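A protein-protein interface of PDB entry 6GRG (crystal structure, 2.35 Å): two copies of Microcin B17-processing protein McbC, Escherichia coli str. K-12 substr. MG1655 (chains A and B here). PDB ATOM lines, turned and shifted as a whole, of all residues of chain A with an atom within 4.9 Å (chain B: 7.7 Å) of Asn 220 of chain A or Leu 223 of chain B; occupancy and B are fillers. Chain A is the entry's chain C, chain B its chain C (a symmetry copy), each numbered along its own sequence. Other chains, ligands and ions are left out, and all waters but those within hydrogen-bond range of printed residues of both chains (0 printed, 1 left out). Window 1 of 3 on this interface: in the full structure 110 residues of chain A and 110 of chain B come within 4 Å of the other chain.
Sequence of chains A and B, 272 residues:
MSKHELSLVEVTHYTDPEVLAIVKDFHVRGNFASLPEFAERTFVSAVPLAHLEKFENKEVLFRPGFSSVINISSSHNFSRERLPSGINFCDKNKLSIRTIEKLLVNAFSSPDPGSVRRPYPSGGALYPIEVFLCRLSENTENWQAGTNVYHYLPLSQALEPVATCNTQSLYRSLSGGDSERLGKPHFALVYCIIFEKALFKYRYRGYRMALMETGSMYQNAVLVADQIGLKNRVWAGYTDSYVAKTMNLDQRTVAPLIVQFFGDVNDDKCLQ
Ser 216 of chain A touches its own counterpart, Ser 216 of chain B. Ser 216 of chain A touches Gln 219 of chain B, and with the chains exchanged Gln 219 of chain A touches Ser 216 of chain B. Gln 219 of chain A touches Asn 220 of chain B, and with the chains exchanged Asn 220 of chain A touches Gln 219 of chain B. Asn 220 of chain A touches Leu 223 of chain B, and with the chains exchanged Leu 223 of chain A touches Asn 220 of chain B. 11 positions are printed for both chains. Of the 13 pairs that touch across the chains among the printed residues, 8 have their exchanged pair printed and touching as well.
Of chain B, only Gln 219 (2.6 Å) and Leu 223 (3.6 Å) come within 4 Å of Asn 220 of chain A. Of chain A, only Asn 220 and Leu 223 come within 4 Å of Leu 223 of chain B. Printed residues of chain A within 4 Å of Asn 220 of chain B: Gln 219 and Leu 223. Of the printed residues of chain B, Gln 219 of chain A touches Ser 216 (3.5 Å) and Asn 220 (2.6 Å). Of the printed residues of chain B, Pro 119 of chain A touches Arg 82 (3.5 Å) and Gln 219 (2.9 Å). Printed residues of chain A within 4 Å of Ser 216 of chain B: Ser 216 and Gln 219. Of the printed residues of chain A, Gly 215 of chain B touches Ser 216 (3.4 Å). Val 222 of chain A touches none of the printed residues of chain B. Leu 230 of chain B touches none of the printed residues of chain A. The nearest residue of chain B that does not touch Asn 220 of chain A is Asn 220 of chain B (6.4 Å). The nearest residue of chain A that does not touch Leu 223 of chain B is Pro 119 of chain A (4.8 Å). The nearest printed residue of chain A that does not touch Ser 216 of chain B is Tyr 218 of chain A (4.1 Å).
Of the 24 printed residues of chain B, 6 touch a printed residue of chain A. Printed residues of chain B that touch a printed residue of chain A: Arg 82, Gly 215, Ser 216, Gln 219, Asn 220 and Leu 223. Hydrophobic or aromatic side chains of chain B that line the printed part of chain A: Leu 223. Printed residues of chain A that touch a printed residue of chain B: Pro 119, Tyr 120, Ser 216, Gln 219, Asn 220 and Leu 223.
Among the printed residues, merely in contact across the chains: Pro 119 of chain A with Arg 82 of chain B (3.5 Å), Tyr 120 of chain A with Gln 219 of chain B (3.7 Å), Ser 216 of chain A with Gly 215 of chain B (3.4 Å), Ser 216 of chain A with Ser 216 of chain B (3.9 Å), Ser 216 of chain A with Gln 219 of chain B (3.5 Å), Gln 219 of chain A with Ser 216 of chain B (3.5 Å), Asn 220 of chain A with Leu 223 of chain B (3.6 Å), Leu 223 of chain A with Asn 220 of chain B (3.6 Å) and Leu 223 of chain A with Leu 223 of chain B (3.5 Å).
O of Pro 119 of chain A sits at hydrogen-bond distance from NE2 of Gln 219 of chain B, at 2.9 Å. O of Tyr 120 of chain A is in hydrogen-bond range of NH2 of Arg 82 of chain B, 3.3 Å away. The side-chain amide oxygen (OD1) of Asn 220 of chain A is in hydrogen-bond range of the side-chain amide nitrogen (NE2) of Gln 219 of chain B, at 2.6 Å. The side-chain amide nitrogen (NE2) of Gln 219 of chain A is in hydrogen-bond range of the side-chain amide oxygen (OD1) of Asn 220 of chain B, at 2.6 Å.
ND2 of Asn 220 of chain A sits at hydrogen-bond distance from O of Pro 119 of chain A (3.0 Å). The backbone carbonyl oxygen (O) of Leu 223 of chain B is in hydrogen-bond range of the side-chain amide nitrogen (NE2) of Gln 227 of chain B (3.1 Å). The side-chain amide nitrogen (ND2) of Asn 220 of chain B sits at hydrogen-bond distance from the backbone carbonyl oxygen (O) of Ala 107 of chain B, 2.9 Å away. O of Ala 107 of chain A sits at hydrogen-bond distance from ND2 of Asn 220 of chain A (2.9 Å). SD of Met 217 of chain A lies close to OH of Tyr 120 of chain A (3.8 Å).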
ATOM      1  N   ALA A 107      -2.916   7.297   0.106  1.00  0.00           N
ATOM      2  CA  ALA A 107      -2.582   5.992  -0.469  1.00  0.00           C
ATOM      3  C   ALA A 107      -3.791   5.362  -1.178  1.00  0.00           C
ATOM      4  O   ALA A 107      -3.600   4.652  -2.173  1.00  0.00           O
ATOM      5  CB  ALA A 107      -2.049   5.053   0.589  1.00  0.00           C
ATOM      6  N   PRO A 119      -6.693   5.806  -6.338  1.00  0.00           N
ATOM      7  CA  PRO A 119      -5.345   5.939  -6.894  1.00  0.00           C
ATOM      8  C   PRO A 119      -4.627   4.616  -7.225  1.00  0.00           C
ATOM      9  O   PRO A 119      -3.427   4.585  -7.313  1.00  0.00           O
ATOM     10  CB  PRO A 119      -4.596   6.706  -5.784  1.00  0.00           C
ATOM     11  CG  PRO A 119      -5.278   6.288  -4.518  1.00  0.00           C
ATOM     12  CD  PRO A 119      -6.733   6.161  -4.913  1.00  0.00           C
ATOM     13  N   TYR A 120      -5.368   3.522  -7.374  1.00  0.00           N
ATOM     14  CA  TYR A 120      -4.822   2.273  -7.899  1.00  0.00           C
ATOM     15  C   TYR A 120      -5.927   1.604  -8.692  1.00  0.00           C
ATOM     16  O   TYR A 120      -7.112   1.785  -8.399  1.00  0.00           O
ATOM     17  CB  TYR A 120      -4.275   1.374  -6.793  1.00  0.00           C
ATOM     18  CG  TYR A 120      -5.280   1.015  -5.726  1.00  0.00           C
ATOM     19  CD1 TYR A 120      -5.543   1.869  -4.666  1.00  0.00           C
ATOM     20  CD2 TYR A 120      -6.008  -0.166  -5.804  1.00  0.00           C
ATOM     21  CE1 TYR A 120      -6.485   1.547  -3.704  1.00  0.00           C
ATOM     22  CE2 TYR A 120      -6.940  -0.511  -4.842  1.00  0.00           C
ATOM     23  CZ  TYR A 120      -7.175   0.349  -3.789  1.00  0.00           C
ATOM     24  OH  TYR A 120      -8.101   0.011  -2.851  1.00  0.00           O
ATOM     25  N   SER A 216      -0.224  -3.140  -5.310  1.00  0.00           N
ATOM     26  CA  SER A 216      -0.403  -1.770  -5.805  1.00  0.00           C
ATOM     27  C   SER A 216      -0.767  -0.885  -4.623  1.00  0.00           C
ATOM     28  O   SER A 216      -0.347   0.288  -4.548  1.00  0.00           O
ATOM     29  CB  SER A 216      -1.432  -1.659  -6.913  1.00  0.00           C
ATOM     30  OG  SER A 216      -2.733  -1.980  -6.455  1.00  0.00           O
ATOM     31  N   MET A 217      -1.530  -1.470  -3.693  1.00  0.00           N
ATOM     32  CA  MET A 217      -2.013  -0.727  -2.561  1.00  0.00           C
ATOM     33  C   MET A 217      -0.880  -0.456  -1.578  1.00  0.00           C
ATOM     34  O   MET A 217      -0.632   0.718  -1.290  1.00  0.00           O
ATOM     35  CB  MET A 217      -3.149  -1.440  -1.848  1.00  0.00           C
ATOM     36  CG  MET A 217      -4.373  -1.514  -2.719  1.00  0.00           C
ATOM     37  SD  MET A 217      -5.544  -2.655  -2.014  1.00  0.00           S
ATOM     38  CE  MET A 217      -6.146  -1.727  -0.605  1.00  0.00           C
ATOM     39  N   TYR A 218      -0.179  -1.500  -1.099  1.00  0.00           N
ATOM     40  CA  TYR A 218       0.807  -1.218  -0.109  1.00  0.00           C
ATOM     41  C   TYR A 218       1.925  -0.347  -0.699  1.00  0.00           C
ATOM     42  O   TYR A 218       2.548   0.372   0.038  1.00  0.00           O
ATOM     43  CB  TYR A 218       1.288  -2.479   0.602  1.00  0.00           C
ATOM     44  CG  TYR A 218       2.163  -3.433  -0.158  1.00  0.00           C
ATOM     45  CD1 TYR A 218       3.331  -3.026  -0.783  1.00  0.00           C
ATOM     46  CD2 TYR A 218       1.874  -4.787  -0.141  1.00  0.00           C
ATOM     47  CE1 TYR A 218       4.155  -3.940  -1.431  1.00  0.00           C
ATOM     48  CE2 TYR A 218       2.671  -5.707  -0.802  1.00  0.00           C
ATOM     49  CZ  TYR A 218       3.821  -5.289  -1.452  1.00  0.00           C
ATOM     50  OH  TYR A 218       4.621  -6.211  -2.073  1.00  0.00           O
ATOM     51  N   GLN A 219       2.132  -0.381  -2.021  1.00  0.00           N
ATOM     52  CA  GLN A 219       3.137   0.432  -2.674  1.00  0.00           C
ATOM     53  C   GLN A 219       2.765   1.913  -2.555  1.00  0.00           C
ATOM     54  O   GLN A 219       3.599   2.707  -2.229  1.00  0.00           O
ATOM     55  CB  GLN A 219       3.306   0.048  -4.151  1.00  0.00           C
ATOM     56  CG  GLN A 219       4.370   0.869  -4.897  1.00  0.00           C
ATOM     57  CD  GLN A 219       5.793   0.733  -4.378  1.00  0.00           C
ATOM     58  OE1 GLN A 219       6.127  -0.162  -3.588  1.00  0.00           O
ATOM     59  NE2 GLN A 219       6.664   1.620  -4.839  1.00  0.00           N
ATOM     60  N   ASN A 220       1.524   2.275  -2.873  1.00  0.00           N
ATOM     61  CA  ASN A 220       1.050   3.657  -2.661  1.00  0.00           C
ATOM     62  C   ASN A 220       1.363   4.072  -1.218  1.00  0.00           C
ATOM     63  O   ASN A 220       1.697   5.254  -0.965  1.00  0.00           O
ATOM     64  CB  ASN A 220      -0.452   3.861  -2.913  1.00  0.00           C
ATOM     65  CG  ASN A 220      -0.823   4.067  -4.364  1.00  0.00           C
ATOM     66  OD1 ASN A 220       0.043   4.048  -5.232  1.00  0.00           O
ATOM     67  ND2 ASN A 220      -2.108   4.250  -4.631  1.00  0.00           N
ATOM     68  N   ALA A 221       1.214   3.126  -0.276  1.00  0.00           N
ATOM     69  CA  ALA A 221       1.411   3.441   1.153  1.00  0.00           C
ATOM     70  C   ALA A 221       2.901   3.736   1.412  1.00  0.00           C
ATOM     71  O   ALA A 221       3.257   4.681   2.108  1.00  0.00           O
ATOM     72  CB  ALA A 221       0.869   2.335   2.032  1.00  0.00           C
ATOM     73  N   VAL A 222       3.762   2.950   0.773  1.00  0.00           N
ATOM     74  CA  VAL A 222       5.203   3.108   0.854  1.00  0.00           C
ATOM     75  C   VAL A 222       5.579   4.526   0.397  1.00  0.00           C
ATOM     76  O   VAL A 222       6.253   5.303   1.122  1.00  0.00           O
ATOM     77  CB  VAL A 222       5.887   2.011   0.020  1.00  0.00           C
ATOM     78  CG1 VAL A 222       7.371   2.280  -0.178  1.00  0.00           C
ATOM     79  CG2 VAL A 222       5.645   0.633   0.631  1.00  0.00           C
ATOM     80  N   LEU A 223       5.093   4.893  -0.793  1.00  0.00           N
ATOM     81  CA  LEU A 223       5.445   6.175  -1.387  1.00  0.00           C
ATOM     82  C   LEU A 223       4.898   7.316  -0.534  1.00  0.00           C
ATOM     83  O   LEU A 223       5.563   8.330  -0.396  1.00  0.00           O
ATOM     84  CB  LEU A 223       4.920   6.226  -2.818  1.00  0.00           C
ATOM     85  CG  LEU A 223       5.556   5.191  -3.742  1.00  0.00           C
ATOM     86  CD1 LEU A 223       4.865   5.173  -5.097  1.00  0.00           C
ATOM     87  CD2 LEU A 223       7.044   5.455  -3.882  1.00  0.00           C
ATOM     88  N   VAL A 224       3.719   7.114   0.070  1.00  0.00           N
ATOM     89  CA  VAL A 224       3.036   8.173   0.794  1.00  0.00           C
ATOM     90  C   VAL A 224       3.730   8.347   2.149  1.00  0.00           C
ATOM     91  O   VAL A 224       3.968   9.497   2.580  1.00  0.00           O
ATOM     92  CB  VAL A 224       1.510   7.930   0.882  1.00  0.00           C
ATOM     93  CG1 VAL A 224       0.806   8.807   1.914  1.00  0.00           C
ATOM     94  CG2 VAL A 224       0.861   8.131  -0.481  1.00  0.00           C
ATOM     95  N   ALA A 225       4.094   7.217   2.770  1.00  0.00           N
ATOM     96  CA  ALA A 225       4.857   7.164   4.031  1.00  0.00           C
ATOM     97  C   ALA A 225       6.166   7.943   3.889  1.00  0.00           C
ATOM     98  O   ALA A 225       6.511   8.786   4.730  1.00  0.00           O
ATOM     99  CB  ALA A 225       5.113   5.720   4.400  1.00  0.00           C
ATOM    100  N   ARG B  80      -2.622  14.153  -6.611  1.00  0.00           N
ATOM    101  CA  ARG B  80      -3.398  14.324  -7.837  1.00  0.00           C
ATOM    102  C   ARG B  80      -4.284  13.078  -7.993  1.00  0.00           C
ATOM    103  O   ARG B  80      -3.916  12.003  -7.540  1.00  0.00           O
ATOM    104  CB  ARG B  80      -2.476  14.504  -9.059  1.00  0.00           C
ATOM    105  CG  ARG B  80      -1.932  15.916  -9.269  1.00  0.00           C
ATOM    106  N   GLU B  81      -5.447  13.217  -8.638  1.00  0.00           N
ATOM    107  CA  GLU B  81      -6.249  12.063  -8.986  1.00  0.00           C
ATOM    108  C   GLU B  81      -5.526  11.289 -10.092  1.00  0.00           C
ATOM    109  O   GLU B  81      -4.974  11.878 -11.005  1.00  0.00           O
ATOM    110  CB  GLU B  81      -7.654  12.449  -9.433  1.00  0.00           C
ATOM    111  CG  GLU B  81      -8.669  11.338  -9.210  1.00  0.00           C
ATOM    112  CD  GLU B  81     -10.109  11.808  -9.335  1.00  0.00           C
ATOM    113  OE1 GLU B  81     -10.440  12.394 -10.385  1.00  0.00           O
ATOM    114  OE2 GLU B  81     -10.889  11.623  -8.375  1.00  0.00           O
ATOM    115  N   ARG B  82      -5.532   9.958  -9.976  1.00  0.00           N
ATOM    116  CA  ARG B  82      -4.990   9.079 -11.011  1.00  0.00           C
ATOM    117  C   ARG B  82      -5.810   9.311 -12.285  1.00  0.00           C
ATOM    118  O   ARG B  82      -7.028   9.502 -12.218  1.00  0.00           O
ATOM    119  CB  ARG B  82      -4.995   7.631 -10.507  1.00  0.00           C
ATOM    120  CG  ARG B  82      -4.501   6.592 -11.498  1.00  0.00           C
ATOM    121  CD  ARG B  82      -4.563   5.185 -10.937  1.00  0.00           C
ATOM    122  NE  ARG B  82      -5.899   4.847 -10.498  1.00  0.00           N
ATOM    123  CZ  ARG B  82      -6.814   4.225 -11.240  1.00  0.00           C
ATOM    124  NH1 ARG B  82      -6.531   3.859 -12.480  1.00  0.00           N
ATOM    125  NH2 ARG B  82      -8.011   3.973 -10.737  1.00  0.00           N
ATOM    126  N   LEU B 103      10.330   5.993 -18.243  1.00  0.00           N
ATOM    127  CA  LEU B 103       9.419   5.163 -17.501  1.00  0.00           C
ATOM    128  C   LEU B 103      10.202   4.071 -16.751  1.00  0.00           C
ATOM    129  O   LEU B 103       9.999   3.837 -15.544  1.00  0.00           O
ATOM    130  CB  LEU B 103       8.392   4.556 -18.460  1.00  0.00           C
ATOM    131  CG  LEU B 103       7.492   3.490 -17.839  1.00  0.00           C
ATOM    132  CD1 LEU B 103       6.472   4.124 -16.908  1.00  0.00           C
ATOM    133  CD2 LEU B 103       6.791   2.662 -18.904  1.00  0.00           C
ATOM    134  N   ALA B 107      10.245   3.902 -12.683  1.00  0.00           N
ATOM    135  CA  ALA B 107       9.363   2.911 -12.063  1.00  0.00           C
ATOM    136  C   ALA B 107      10.164   1.829 -11.319  1.00  0.00           C
ATOM    137  O   ALA B 107       9.682   1.321 -10.300  1.00  0.00           O
ATOM    138  CB  ALA B 107       8.454   2.274 -13.089  1.00  0.00           C
ATOM    139  N   GLY B 215       2.357  -6.264  -8.327  1.00  0.00           N
ATOM    140  CA  GLY B 215       1.455  -5.140  -8.202  1.00  0.00           C
ATOM    141  C   GLY B 215       2.175  -3.863  -7.796  1.00  0.00           C
ATOM    142  O   GLY B 215       1.790  -2.781  -8.265  1.00  0.00           O
ATOM    143  N   SER B 216       3.179  -3.984  -6.903  1.00  0.00           N
ATOM    144  CA  SER B 216       3.962  -2.825  -6.459  1.00  0.00           C
ATOM    145  C   SER B 216       4.676  -2.244  -7.669  1.00  0.00           C
ATOM    146  O   SER B 216       4.830  -1.012  -7.793  1.00  0.00           O
ATOM    147  CB  SER B 216       4.940  -3.149  -5.347  1.00  0.00           C
ATOM    148  OG  SER B 216       5.952  -4.040  -5.780  1.00  0.00           O
ATOM    149  N   MET B 217       5.084  -3.145  -8.570  1.00  0.00           N
ATOM    150  CA  MET B 217       5.840  -2.744  -9.724  1.00  0.00           C
ATOM    151  C   MET B 217       4.943  -2.028 -10.727  1.00  0.00           C
ATOM    152  O   MET B 217       5.249  -0.879 -11.062  1.00  0.00           O
ATOM    153  CB  MET B 217       6.525  -3.920 -10.400  1.00  0.00           C
ATOM    154  CG  MET B 217       7.593  -4.505  -9.517  1.00  0.00           C
ATOM    155  SD  MET B 217       8.115  -6.077 -10.167  1.00  0.00           S
ATOM    156  CE  MET B 217       9.059  -5.575 -11.605  1.00  0.00           C
ATOM    157  N   TYR B 218       3.842  -2.660 -11.173  1.00  0.00           N
ATOM    158  CA  TYR B 218       3.081  -2.000 -12.182  1.00  0.00           C
ATOM    159  C   TYR B 218       2.482  -0.697 -11.635  1.00  0.00           C
ATOM    160  O   TYR B 218       2.244   0.198 -12.404  1.00  0.00           O
ATOM    161  CB  TYR B 218       2.076  -2.934 -12.850  1.00  0.00           C
ATOM    162  CG  TYR B 218       0.872  -3.361 -12.062  1.00  0.00           C
ATOM    163  CD1 TYR B 218       0.019  -2.447 -11.464  1.00  0.00           C
ATOM    164  CD2 TYR B 218       0.517  -4.699 -12.026  1.00  0.00           C
ATOM    165  CE1 TYR B 218      -1.124  -2.865 -10.789  1.00  0.00           C
ATOM    166  CE2 TYR B 218      -0.603  -5.134 -11.337  1.00  0.00           C
ATOM    167  CZ  TYR B 218      -1.434  -4.218 -10.714  1.00  0.00           C
ATOM    168  OH  TYR B 218      -2.559  -4.655 -10.066  1.00  0.00           O
ATOM    169  N   GLN B 219       2.294  -0.584 -10.314  1.00  0.00           N
ATOM    170  CA  GLN B 219       1.770   0.619  -9.701  1.00  0.00           C
ATOM    171  C   GLN B 219       2.769   1.767  -9.873  1.00  0.00           C
ATOM    172  O   GLN B 219       2.381   2.839 -10.236  1.00  0.00           O
ATOM    173  CB  GLN B 219       1.459   0.408  -8.213  1.00  0.00           C
ATOM    174  CG  GLN B 219       0.887   1.648  -7.507  1.00  0.00           C
ATOM    175  CD  GLN B 219      -0.449   2.150  -8.034  1.00  0.00           C
ATOM    176  OE1 GLN B 219      -1.158   1.474  -8.792  1.00  0.00           O
ATOM    177  NE2 GLN B 219      -0.821   3.352  -7.615  1.00  0.00           N
ATOM    178  N   ASN B 220       4.043   1.541  -9.557  1.00  0.00           N
ATOM    179  CA  ASN B 220       5.088   2.552  -9.817  1.00  0.00           C
ATOM    180  C   ASN B 220       4.983   3.008 -11.277  1.00  0.00           C
ATOM    181  O   ASN B 220       5.216   4.203 -11.577  1.00  0.00           O
ATOM    182  CB  ASN B 220       6.523   2.064  -9.559  1.00  0.00           C
ATOM    183  CG  ASN B 220       6.959   2.135  -8.114  1.00  0.00           C
ATOM    184  OD1 ASN B 220       6.186   2.542  -7.254  1.00  0.00           O
ATOM    185  ND2 ASN B 220       8.191   1.728  -7.843  1.00  0.00           N
ATOM    186  N   ALA B 221       4.680   2.062 -12.181  1.00  0.00           N
ATOM    187  CA  ALA B 221       4.634   2.379 -13.623  1.00  0.00           C
ATOM    188  C   ALA B 221       3.436   3.304 -13.907  1.00  0.00           C
ATOM    189  O   ALA B 221       3.538   4.282 -14.640  1.00  0.00           O
ATOM    190  CB  ALA B 221       4.610   1.115 -14.455  1.00  0.00           C
ATOM    191  N   VAL B 222       2.318   3.016 -13.246  1.00  0.00           N
ATOM    192  CA  VAL B 222       1.103   3.805 -13.346  1.00  0.00           C
ATOM    193  C   VAL B 222       1.412   5.256 -12.945  1.00  0.00           C
ATOM    194  O   VAL B 222       1.155   6.225 -13.705  1.00  0.00           O
ATOM    195  CB  VAL B 222       0.005   3.167 -12.478  1.00  0.00           C
ATOM    196  CG1 VAL B 222      -1.196   4.084 -12.303  1.00  0.00           C
ATOM    197  CG2 VAL B 222      -0.406   1.806 -13.034  1.00  0.00           C
ATOM    198  N   LEU B 223       2.022   5.408 -11.767  1.00  0.00           N
ATOM    199  CA  LEU B 223       2.292   6.732 -11.224  1.00  0.00           C
ATOM    200  C   LEU B 223       3.288   7.470 -12.115  1.00  0.00           C
ATOM    201  O   LEU B 223       3.150   8.670 -12.296  1.00  0.00           O
ATOM    202  CB  LEU B 223       2.796   6.594  -9.791  1.00  0.00           C
ATOM    203  CG  LEU B 223       1.769   5.993  -8.834  1.00  0.00           C
ATOM    204  CD1 LEU B 223       2.390   5.717  -7.474  1.00  0.00           C
ATOM    205  CD2 LEU B 223       0.563   6.906  -8.718  1.00  0.00           C
ATOM    206  N   VAL B 224       4.243   6.735 -12.699  1.00  0.00           N
ATOM    207  CA  VAL B 224       5.324   7.344 -13.457  1.00  0.00           C
ATOM    208  C   VAL B 224       4.771   7.762 -14.823  1.00  0.00           C
ATOM    209  O   VAL B 224       5.075   8.878 -15.299  1.00  0.00           O
ATOM    210  CB  VAL B 224       6.575   6.435 -13.521  1.00  0.00           C
ATOM    211  CG1 VAL B 224       7.590   6.860 -14.580  1.00  0.00           C
ATOM    212  CG2 VAL B 224       7.257   6.373 -12.162  1.00  0.00           C
ATOM    213  N   ALA B 225       3.931   6.896 -15.405  1.00  0.00           N
ATOM    214  CA  ALA B 225       3.215   7.145 -16.670  1.00  0.00           C
ATOM    215  C   ALA B 225       2.399   8.436 -16.569  1.00  0.00           C
ATOM    216  O   ALA B 225       2.465   9.312 -17.444  1.00  0.00           O
ATOM    217  CB  ALA B 225       2.331   5.960 -16.987  1.00  0.00           C
ATOM    218  N   ASP B 226       1.648   8.562 -15.473  1.00  0.00           N
ATOM    219  CA  ASP B 226       0.818   9.750 -15.266  1.00  0.00           C
ATOM    220  C   ASP B 226       1.703  11.002 -15.311  1.00  0.00           C
ATOM    221  O   ASP B 226       1.344  12.005 -15.938  1.00  0.00           O
ATOM    222  CB  ASP B 226      -0.003   9.644 -13.975  1.00  0.00           C
ATOM    223  CG  ASP B 226      -1.262   8.791 -14.090  1.00  0.00           C
ATOM    224  OD1 ASP B 226      -1.293   7.848 -14.917  1.00  0.00           O
ATOM    225  OD2 ASP B 226      -2.213   9.076 -13.356  1.00  0.00           O
ATOM    226  N   GLN B 227       2.874  10.927 -14.667  1.00  0.00           N
ATOM    227  CA  GLN B 227       3.770  12.087 -14.495  1.00  0.00           C
ATOM    228  C   GLN B 227       4.469  12.453 -15.807  1.00  0.00           C
ATOM    229  O   GLN B 227       4.750  13.606 -16.008  1.00  0.00           O
ATOM    230  CB  GLN B 227       4.846  11.834 -13.443  1.00  0.00           C
ATOM    231  CG  GLN B 227       4.345  11.820 -12.007  1.00  0.00           C
ATOM    232  CD  GLN B 227       5.441  11.365 -11.071  1.00  0.00           C
ATOM    233  OE1 GLN B 227       6.144  12.174 -10.472  1.00  0.00           O
ATOM    234  NE2 GLN B 227       5.628  10.061 -10.969  1.00  0.00           N
ATOM    235  N   ILE B 228       4.761  11.496 -16.690  1.00  0.00           N
ATOM    236  CA  ILE B 228       5.443  11.854 -17.956  1.00  0.00           C
ATOM    237  C   ILE B 228       4.437  11.971 -19.110  1.00  0.00           C
ATOM    238  O   ILE B 228       4.850  12.115 -20.255  1.00  0.00           O
ATOM    239  CB  ILE B 228       6.576  10.860 -18.291  1.00  0.00           C
ATOM    240  CG1 ILE B 228       6.042   9.460 -18.612  1.00  0.00           C
ATOM    241  CG2 ILE B 228       7.625  10.834 -17.182  1.00  0.00           C
ATOM    242  CD1 ILE B 228       7.127   8.458 -18.891  1.00  0.00           C
ATOM    243  N   GLY B 229       3.129  11.886 -18.819  1.00  0.00           N
ATOM    244  CA  GLY B 229       2.068  12.162 -19.810  1.00  0.00           C
ATOM    245  C   GLY B 229       1.850  11.016 -20.792  1.00  0.00           C
ATOM    246  O   GLY B 229       1.565  11.268 -21.951  1.00  0.00           O
ATOM    247  N   LEU B 230       2.009   9.768 -20.313  1.00  0.00           N
ATOM    248  CA  LEU B 230       1.679   8.527 -21.003  1.00  0.00           C
ATOM    249  C   LEU B 230       0.344   8.022 -20.443  1.00  0.00           C
ATOM    250  O   LEU B 230       0.158   8.082 -19.232  1.00  0.00           O
ATOM    251  CB  LEU B 230       2.733   7.468 -20.664  1.00  0.00           C
ATOM    252  CG  LEU B 230       3.878   7.226 -21.639  1.00  0.00           C
ATOM    253  CD1 LEU B 230       4.680   6.031 -21.153  1.00  0.00           C
ATOM    254  CD2 LEU B 230       3.384   6.976 -23.052  1.00  0.00           C
ATOM    255  N   ASN B 232      -2.034   4.505 -19.783  1.00  0.00           N
ATOM    256  CA  ASN B 232      -1.739   3.107 -19.593  1.00  0.00           C
ATOM    257  C   ASN B 232      -2.982   2.333 -19.142  1.00  0.00           C
ATOM    258  O   ASN B 232      -3.972   2.898 -18.641  1.00  0.00           O
ATOM    259  CB  ASN B 232      -0.638   2.898 -18.559  1.00  0.00           C
ATOM    260  CG  ASN B 232      -1.157   2.965 -17.142  1.00  0.00           C
ATOM    261  OD1 ASN B 232      -1.362   1.940 -16.506  1.00  0.00           O
ATOM    262  ND2 ASN B 232      -1.385   4.166 -16.650  1.00  0.00           N
ATOM    263  N   GLN B 260       0.792  -4.712 -19.192  1.00  0.00           N
ATOM    264  CA  GLN B 260       0.453  -3.331 -18.996  1.00  0.00           C
ATOM    265  C   GLN B 260       0.718  -2.564 -20.295  1.00  0.00           C
ATOM    266  O   GLN B 260       1.854  -2.551 -20.788  1.00  0.00           O
ATOM    267  CB  GLN B 260       1.233  -2.759 -17.812  1.00  0.00           C
ATOM    268  CG  GLN B 260       0.861  -1.312 -17.545  1.00  0.00           C
ATOM    269  CD  GLN B 260       1.478  -0.708 -16.311  1.00  0.00           C
ATOM    270  OE1 GLN B 260       2.497  -1.183 -15.794  1.00  0.00           O
ATOM    271  NE2 GLN B 260       0.848   0.365 -15.847  1.00  0.00           N
ATOM    272  N   PHE B 262       0.770   0.918 -22.812  1.00  0.00           N
ATOM    273  CA  PHE B 262       1.187   2.337 -22.766  1.00  0.00           C
ATOM    274  C   PHE B 262       1.067   3.022 -24.144  1.00  0.00           C
ATOM    275  O   PHE B 262       1.342   2.420 -25.202  1.00  0.00           O
ATOM    276  CB  PHE B 262       2.631   2.458 -22.266  1.00  0.00           C
ATOM    277  CG  PHE B 262       2.855   1.917 -20.879  1.00  0.00           C
ATOM    278  CD1 PHE B 262       3.181   0.583 -20.677  1.00  0.00           C
ATOM    279  CD2 PHE B 262       2.727   2.740 -19.774  1.00  0.00           C
ATOM    280  CE1 PHE B 262       3.382   0.098 -19.401  1.00  0.00           C
ATOM    281  CE2 PHE B 262       2.926   2.243 -18.495  1.00  0.00           C
ATOM    282  CZ  PHE B 262       3.263   0.932 -18.317  1.00  0.00           C
